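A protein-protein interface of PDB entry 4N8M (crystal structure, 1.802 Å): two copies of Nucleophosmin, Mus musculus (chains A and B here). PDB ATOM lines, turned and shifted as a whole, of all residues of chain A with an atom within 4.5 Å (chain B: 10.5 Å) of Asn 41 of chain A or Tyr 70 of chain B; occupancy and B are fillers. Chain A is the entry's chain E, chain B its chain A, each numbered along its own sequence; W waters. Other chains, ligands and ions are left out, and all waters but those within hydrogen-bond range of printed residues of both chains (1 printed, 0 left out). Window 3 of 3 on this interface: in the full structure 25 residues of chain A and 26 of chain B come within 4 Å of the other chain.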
ATOM      1  N   TYR A  20       5.081  26.228 -22.132  1.00  0.00           N
ATOM      2  CA  TYR A  20       4.595  26.340 -20.767  1.00  0.00           C
ATOM      3  C   TYR A  20       4.611  27.783 -20.321  1.00  0.00           C
ATOM      4  O   TYR A  20       5.414  28.587 -20.792  1.00  0.00           O
ATOM      5  CB  TYR A  20       5.467  25.504 -19.807  1.00  0.00           C
ATOM      6  CG  TYR A  20       5.534  24.054 -20.223  1.00  0.00           C
ATOM      7  CD1 TYR A  20       6.535  23.602 -21.069  1.00  0.00           C
ATOM      8  CD2 TYR A  20       4.565  23.146 -19.800  1.00  0.00           C
ATOM      9  CE1 TYR A  20       6.583  22.270 -21.467  1.00  0.00           C
ATOM     10  CE2 TYR A  20       4.603  21.827 -20.192  1.00  0.00           C
ATOM     11  CZ  TYR A  20       5.610  21.393 -21.024  1.00  0.00           C
ATOM     12  OH  TYR A  20       5.637  20.076 -21.413  1.00  0.00           O
ATOM     13  N   ASP A  37      17.654  23.304 -16.408  1.00  0.00           N
ATOM     14  CA  ASP A  37      16.917  22.163 -15.878  1.00  0.00           C
ATOM     15  C   ASP A  37      17.767  20.890 -15.873  1.00  0.00           C
ATOM     16  O   ASP A  37      18.722  20.759 -16.642  1.00  0.00           O
ATOM     17  CB  ASP A  37      15.606  21.958 -16.647  1.00  0.00           C
ATOM     18  CG  ASP A  37      14.576  23.047 -16.349  1.00  0.00           C
ATOM     19  OD1 ASP A  37      13.837  22.913 -15.348  1.00  0.00           O
ATOM     20  OD2 ASP A  37      14.503  24.038 -17.112  1.00  0.00           O
ATOM     21  N   ASP A  39      17.578  18.034 -17.207  1.00  0.00           N
ATOM     22  CA  ASP A  39      17.145  17.137 -18.264  1.00  0.00           C
ATOM     23  C   ASP A  39      17.969  17.435 -19.496  1.00  0.00           C
ATOM     24  O   ASP A  39      18.763  18.375 -19.497  1.00  0.00           O
ATOM     25  CB  ASP A  39      15.653  17.288 -18.559  1.00  0.00           C
ATOM     26  CG  ASP A  39      15.285  18.677 -19.046  1.00  0.00           C
ATOM     27  OD1 ASP A  39      15.864  19.150 -20.050  1.00  0.00           O
ATOM     28  OD2 ASP A  39      14.399  19.294 -18.419  1.00  0.00           O
ATOM     29  N   GLU A  40      17.777  16.639 -20.542  1.00  0.00           N
ATOM     30  CA  GLU A  40      18.606  16.756 -21.733  1.00  0.00           C
ATOM     31  C   GLU A  40      17.848  17.437 -22.864  1.00  0.00           C
ATOM     32  O   GLU A  40      18.231  17.355 -24.031  1.00  0.00           O
ATOM     33  CB  GLU A  40      19.138  15.377 -22.146  1.00  0.00           C
ATOM     34  CG  GLU A  40      20.037  14.758 -21.057  1.00  0.00           C
ATOM     35  CD  GLU A  40      20.528  13.355 -21.376  1.00  0.00           C
ATOM     36  OE1 GLU A  40      20.413  12.918 -22.538  1.00  0.00           O
ATOM     37  OE2 GLU A  40      21.031  12.694 -20.449  1.00  0.00           O
ATOM     38  N   ASN A  41      16.774  18.128 -22.501  1.00  0.00           N
ATOM     39  CA  ASN A  41      15.972  18.856 -23.472  1.00  0.00           C
ATOM     40  C   ASN A  41      16.587  20.221 -23.743  1.00  0.00           C
ATOM     41  O   ASN A  41      17.451  20.682 -22.998  1.00  0.00           O
ATOM     42  CB  ASN A  41      14.542  19.029 -22.954  1.00  0.00           C
ATOM     43  CG  ASN A  41      13.821  17.706 -22.767  1.00  0.00           C
ATOM     44  OD1 ASN A  41      14.022  16.754 -23.533  1.00  0.00           O
ATOM     45  ND2 ASN A  41      12.967  17.640 -21.744  1.00  0.00           N
ATOM     46  N   GLU A  42      16.136  20.864 -24.810  1.00  0.00           N
ATOM     47  CA  GLU A  42      16.567  22.222 -25.120  1.00  0.00           C
ATOM     48  C   GLU A  42      15.537  23.174 -24.527  1.00  0.00           C
ATOM     49  O   GLU A  42      14.340  22.942 -24.665  1.00  0.00           O
ATOM     50  CB  GLU A  42      16.648  22.395 -26.634  1.00  0.00           C
ATOM     51  CG  GLU A  42      17.819  23.227 -27.123  1.00  0.00           C
ATOM     52  CD  GLU A  42      18.143  22.950 -28.582  1.00  0.00           C
ATOM     53  OE1 GLU A  42      17.639  21.938 -29.117  1.00  0.00           O
ATOM     54  OE2 GLU A  42      18.896  23.739 -29.193  1.00  0.00           O
ATOM     55  N   HIS A  43      15.997  24.229 -23.857  1.00  0.00           N
ATOM     56  CA  HIS A  43      15.074  25.158 -23.190  1.00  0.00           C
ATOM     57  C   HIS A  43      15.308  26.596 -23.603  1.00  0.00           C
ATOM     58  O   HIS A  43      16.452  27.017 -23.771  1.00  0.00           O
ATOM     59  CB  HIS A  43      15.231  25.088 -21.668  1.00  0.00           C
ATOM     60  CG  HIS A  43      14.913  23.752 -21.082  1.00  0.00           C
ATOM     61  ND1 HIS A  43      13.742  23.502 -20.401  1.00  0.00           N
ATOM     62  CD2 HIS A  43      15.626  22.598 -21.045  1.00  0.00           C
ATOM     63  CE1 HIS A  43      13.739  22.249 -19.980  1.00  0.00           C
ATOM     64  NE2 HIS A  43      14.871  21.679 -20.358  1.00  0.00           N
ATOM     65  N   HIS A 118       7.916  29.360 -21.145  1.00  0.00           N
ATOM     66  CA  HIS A 118       9.028  28.415 -21.061  1.00  0.00           C
ATOM     67  C   HIS A 118       8.880  27.434 -22.216  1.00  0.00           C
ATOM     68  O   HIS A 118       7.952  26.614 -22.231  1.00  0.00           O
ATOM     69  CB  HIS A 118       9.020  27.700 -19.706  1.00  0.00           C
ATOM     70  CG  HIS A 118      10.164  26.749 -19.511  1.00  0.00           C
ATOM     71  ND1 HIS A 118      10.381  26.077 -18.329  1.00  0.00           N
ATOM     72  CD2 HIS A 118      11.150  26.356 -20.353  1.00  0.00           C
ATOM     73  CE1 HIS A 118      11.448  25.308 -18.447  1.00  0.00           C
ATOM     74  NE2 HIS A 118      11.940  25.465 -19.664  1.00  0.00           N
ATOM     75  N   VAL A 120      10.191  24.289 -24.491  1.00  0.00           N
ATOM     76  CA  VAL A 120      11.016  23.091 -24.358  1.00  0.00           C
ATOM     77  C   VAL A 120      10.966  22.253 -25.623  1.00  0.00           C
ATOM     78  O   VAL A 120       9.890  21.856 -26.071  1.00  0.00           O
ATOM     79  CB  VAL A 120      10.562  22.208 -23.184  1.00  0.00           C
ATOM     80  CG1 VAL A 120      11.567  21.063 -22.959  1.00  0.00           C
ATOM     81  CG2 VAL A 120      10.412  23.040 -21.925  1.00  0.00           C
ATOM     82  N   ALA A 121      12.130  21.988 -26.205  1.00  0.00           N
ATOM     83  CA  ALA A 121      12.192  21.074 -27.342  1.00  0.00           C
ATOM     84  C   ALA A 121      12.572  19.686 -26.844  1.00  0.00           C
ATOM     85  O   ALA A 121      13.667  19.490 -26.313  1.00  0.00           O
ATOM     86  CB  ALA A 121      13.188  21.577 -28.385  1.00  0.00           C
ATOM     87  N   VAL A 122      11.657  18.731 -26.993  1.00  0.00           N
ATOM     88  CA  VAL A 122      11.848  17.392 -26.432  1.00  0.00           C
ATOM     89  C   VAL A 122      12.138  16.349 -27.504  1.00  0.00           C
ATOM     90  O   VAL A 122      13.040  16.517 -28.325  1.00  0.00           O
ATOM     91  CB  VAL A 122      10.621  16.939 -25.615  1.00  0.00           C
ATOM     92  N   ALA B  67      -2.091  29.067 -15.621  1.00  0.00           N
ATOM     93  CA  ALA B  67      -1.945  27.922 -16.515  1.00  0.00           C
ATOM     94  C   ALA B  67      -0.780  27.077 -16.030  1.00  0.00           C
ATOM     95  O   ALA B  67      -0.092  27.456 -15.085  1.00  0.00           O
ATOM     96  CB  ALA B  67      -1.720  28.387 -17.952  1.00  0.00           C
ATOM     97  N   MET B  68      -0.566  25.933 -16.665  1.00  0.00           N
ATOM     98  CA  MET B  68       0.456  24.989 -16.209  1.00  0.00           C
ATOM     99  C   MET B  68       1.894  25.398 -16.553  1.00  0.00           C
ATOM    100  O   MET B  68       2.178  25.850 -17.674  1.00  0.00           O
ATOM    101  CB  MET B  68       0.175  23.601 -16.790  1.00  0.00           C
ATOM    102  CG  MET B  68      -1.149  23.020 -16.345  1.00  0.00           C
ATOM    103  SD  MET B  68      -1.256  22.946 -14.549  1.00  0.00           S
ATOM    104  CE  MET B  68      -3.028  23.117 -14.311  1.00  0.00           C
ATOM    105  N   ASN B  69       2.796  25.230 -15.584  1.00  0.00           N
ATOM    106  CA  ASN B  69       4.222  25.405 -15.837  1.00  0.00           C
ATOM    107  C   ASN B  69       4.861  24.085 -16.287  1.00  0.00           C
ATOM    108  O   ASN B  69       4.175  23.061 -16.392  1.00  0.00           O
ATOM    109  CB  ASN B  69       4.948  25.991 -14.614  1.00  0.00           C
ATOM    110  CG  ASN B  69       5.015  25.017 -13.435  1.00  0.00           C
ATOM    111  OD1 ASN B  69       4.784  23.811 -13.578  1.00  0.00           O
ATOM    112  ND2 ASN B  69       5.346  25.543 -12.263  1.00  0.00           N
ATOM    113  N   TYR B  70       6.163  24.120 -16.567  1.00  0.00           N
ATOM    114  CA  TYR B  70       6.888  22.936 -17.058  1.00  0.00           C
ATOM    115  C   TYR B  70       6.842  21.796 -16.051  1.00  0.00           C
ATOM    116  O   TYR B  70       6.783  20.620 -16.423  1.00  0.00           O
ATOM    117  CB  TYR B  70       8.346  23.293 -17.371  1.00  0.00           C
ATOM    118  CG  TYR B  70       9.188  22.142 -17.888  1.00  0.00           C
ATOM    119  CD1 TYR B  70       8.704  21.286 -18.872  1.00  0.00           C
ATOM    120  CD2 TYR B  70      10.475  21.925 -17.407  1.00  0.00           C
ATOM    121  CE1 TYR B  70       9.473  20.238 -19.356  1.00  0.00           C
ATOM    122  CE2 TYR B  70      11.254  20.879 -17.888  1.00  0.00           C
ATOM    123  CZ  TYR B  70      10.746  20.040 -18.862  1.00  0.00           C
ATOM    124  OH  TYR B  70      11.507  19.000 -19.347  1.00  0.00           O
ATOM    125  N   GLU B  71       6.866  22.146 -14.774  1.00  0.00           N
ATOM    126  CA  GLU B  71       6.896  21.141 -13.718  1.00  0.00           C
ATOM    127  C   GLU B  71       5.544  20.458 -13.530  1.00  0.00           C
ATOM    128  O   GLU B  71       5.451  19.439 -12.852  1.00  0.00           O
ATOM    129  CB  GLU B  71       7.387  21.758 -12.407  1.00  0.00           C
ATOM    130  CG  GLU B  71       8.798  22.328 -12.509  1.00  0.00           C
ATOM    131  CD  GLU B  71       9.303  22.897 -11.196  1.00  0.00           C
ATOM    132  OE1 GLU B  71       8.484  23.453 -10.431  1.00  0.00           O
ATOM    133  OE2 GLU B  71      10.520  22.786 -10.929  1.00  0.00           O
ATOM    134  N   GLY B  72       4.498  21.024 -14.130  1.00  0.00           N
ATOM    135  CA  GLY B  72       3.176  20.424 -14.085  1.00  0.00           C
ATOM    136  C   GLY B  72       2.221  20.948 -13.021  1.00  0.00           C
ATOM    137  O   GLY B  72       1.217  20.306 -12.718  1.00  0.00           O
ATOM    138  N   SER B  73       2.519  22.108 -12.450  1.00  0.00           N
ATOM    139  CA  SER B  73       1.607  22.723 -11.490  1.00  0.00           C
ATOM    140  C   SER B  73       1.101  24.065 -12.015  1.00  0.00           C
ATOM    141  O   SER B  73       1.753  24.687 -12.859  1.00  0.00           O
ATOM    142  CB  SER B  73       2.281  22.893 -10.124  1.00  0.00           C
ATOM    143  OG  SER B  73       3.408  23.745 -10.209  1.00  0.00           O
ATOM    144  N   PRO B  74      -0.066  24.516 -11.522  1.00  0.00           N
ATOM    145  CA  PRO B  74      -0.634  25.767 -12.029  1.00  0.00           C
ATOM    146  C   PRO B  74       0.192  26.933 -11.529  1.00  0.00           C
ATOM    147  O   PRO B  74       0.652  26.913 -10.386  1.00  0.00           O
ATOM    148  CB  PRO B  74      -2.030  25.816 -11.387  1.00  0.00           C
ATOM    149  CG  PRO B  74      -2.237  24.475 -10.743  1.00  0.00           C
ATOM    150  CD  PRO B  74      -0.875  23.955 -10.431  1.00  0.00           C
ATOM    151  N   ILE B  75       0.398  27.930 -12.378  1.00  0.00           N
ATOM    152  CA  ILE B  75       1.075  29.140 -11.929  1.00  0.00           C
ATOM    153  C   ILE B  75       0.307  30.367 -12.372  1.00  0.00           C
ATOM    154  O   ILE B  75      -0.349  30.351 -13.421  1.00  0.00           O
ATOM    155  CB  ILE B  75       2.522  29.227 -12.437  1.00  0.00           C
ATOM    156  CG1 ILE B  75       2.558  29.273 -13.960  1.00  0.00           C
ATOM    157  CG2 ILE B  75       3.343  28.046 -11.919  1.00  0.00           C
ATOM    158  CD1 ILE B  75       3.920  29.608 -14.490  1.00  0.00           C
ATOM    159  N   VAL B  77       0.431  34.377 -13.445  1.00  0.00           N
ATOM    160  CA  VAL B  77       1.349  35.383 -13.964  1.00  0.00           C
ATOM    161  C   VAL B  77       0.577  36.649 -14.314  1.00  0.00           C
ATOM    162  O   VAL B  77      -0.599  36.592 -14.655  1.00  0.00           O
ATOM    163  CB  VAL B  77       2.119  34.878 -15.213  1.00  0.00           C
ATOM    164  CG1 VAL B  77       2.575  33.439 -15.004  1.00  0.00           C
ATOM    165  CG2 VAL B  77       1.259  34.986 -16.467  1.00  0.00           C
ATOM    166  N   THR B  98      -1.090  27.252 -23.666  1.00  0.00           N
ATOM    167  CA  THR B  98      -1.805  25.999 -23.901  1.00  0.00           C
ATOM    168  C   THR B  98      -2.926  25.884 -22.876  1.00  0.00           C
ATOM    169  O   THR B  98      -2.706  26.115 -21.691  1.00  0.00           O
ATOM    170  CB  THR B  98      -0.865  24.794 -23.733  1.00  0.00           C
ATOM    171  OG1 THR B  98       0.293  24.982 -24.554  1.00  0.00           O
ATOM    172  CG2 THR B  98      -1.571  23.516 -24.143  1.00  0.00           C
HETATM  173  O   HOH W   1       7.410  26.701 -16.957  1.00  0.00           O
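OD1 of Asn 69 of chain B is in hydrogen-bond range of N of Glu 71 of chain B.
The backbone NH (N) of Ser 73 of chain B lies within hydrogen-bond range of the side-chain amide oxygen (OD1) of Asn 69 of chain B.
O of Tyr 20 of chain A lies within hydrogen-bond range of N of His 118 of chain A (2.6 Å).
The side-chain carboxylate of Asp 37 of chain A sits at hydrogen-bond distance from a ring nitrogen (ND1) of His 43 of chain A, 3.4 Å away.
OD1 of Asp 39 of chain A is in hydrogen-bond range of N of Asn 41 of chain A, at 2.8 Å.
A ring nitrogen (ND1) of His 43 of chain A sits at hydrogen-bond distance from a ring nitrogen (NE2) of His 118 of chain A, 2.8 Å away.
The side-chain hydroxyl of Tyr 70 of chain B is in hydrogen-bond range of the side-chain carboxylate of Asp 39 of chain A, at 3.1 Å.
The side-chain hydroxyl (OH) of Tyr 70 of chain B sits at hydrogen-bond distance from the side-chain amide nitrogen (ND2) of Asn 41 of chain A (3.1 Å).
Asp 39 of chain A touches just one residue of chain B: Tyr 70 (3.1 Å).
Of chain B, only Tyr 70 comes within 4 Å of Asn 41 of chain A.
Glu 42 of chain A touches none of the printed residues of chain B.
Of the printed residues of chain B, His 43 of chain A touches Tyr 70.
Printed residues of chain B within 4 Å of His 118 of chain A: Tyr 70 (3.6 Å).
Of the printed residues of chain B, Val 120 of chain A touches Tyr 70 (3.9 Å).
No residue of chain B comes within 4 Å of Ala 121 of chain A.
No residue of chain B comes within 4 Å of Val 122 of chain A.
Of the printed residues of chain A, Met 68 of chain B touches Tyr 20 (3.9 Å).
Printed residues of chain A within 4 Å of Asn 69 of chain B: Tyr 20 (3.4 Å).
Tyr 70 of chain B touches just these residues of chain A: Tyr 20 (3.5 Å), Asp 39 (3.1 Å), Asn 41 (3.1 Å), His 43 (3.5 Å), His 118 (3.6 Å) and Val 120 (3.9 Å).
Thr 98 of chain B touches none of the printed residues of chain A.
Among the printed residues, merely in contact across the chains: Tyr 20 of chain A with Asn 69 of chain B (3.4 Å), Tyr 20 of chain A with Tyr 70 of chain B (3.5 Å), His 43 of chain A with Tyr 70 of chain B (3.5 Å), His 118 of chain A with Tyr 70 of chain B (3.6 Å), Val 120 of chain A with Tyr 70 of chain B (3.9 Å) and Tyr 20 of chain A with Met 68 of chain B (3.9 Å).
Of the 11 printed residues of chain A, 6 touch a printed residue of chain B.
Hydrophobic or aromatic side chains of chain A that line the printed part of chain B: Tyr 20, His 43, His 118 and Val 120.
Along chain A the printed residues that touch a printed residue of chain B span positions 20 to 120.
Of the 11 printed residues of chain B, 3 touch a printed residue of chain A.
Hydrophobic or aromatic side chains of chain B that line the printed part of chain A: Tyr 70.
Among the printed residues, 8 pairs touch across the chains.
No position is printed for both chains.
Water W1 lies within hydrogen-bond range of N of Tyr 70 of chain B (2.9 Å) and ND1 of His 118 of chain A (3.3 Å).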
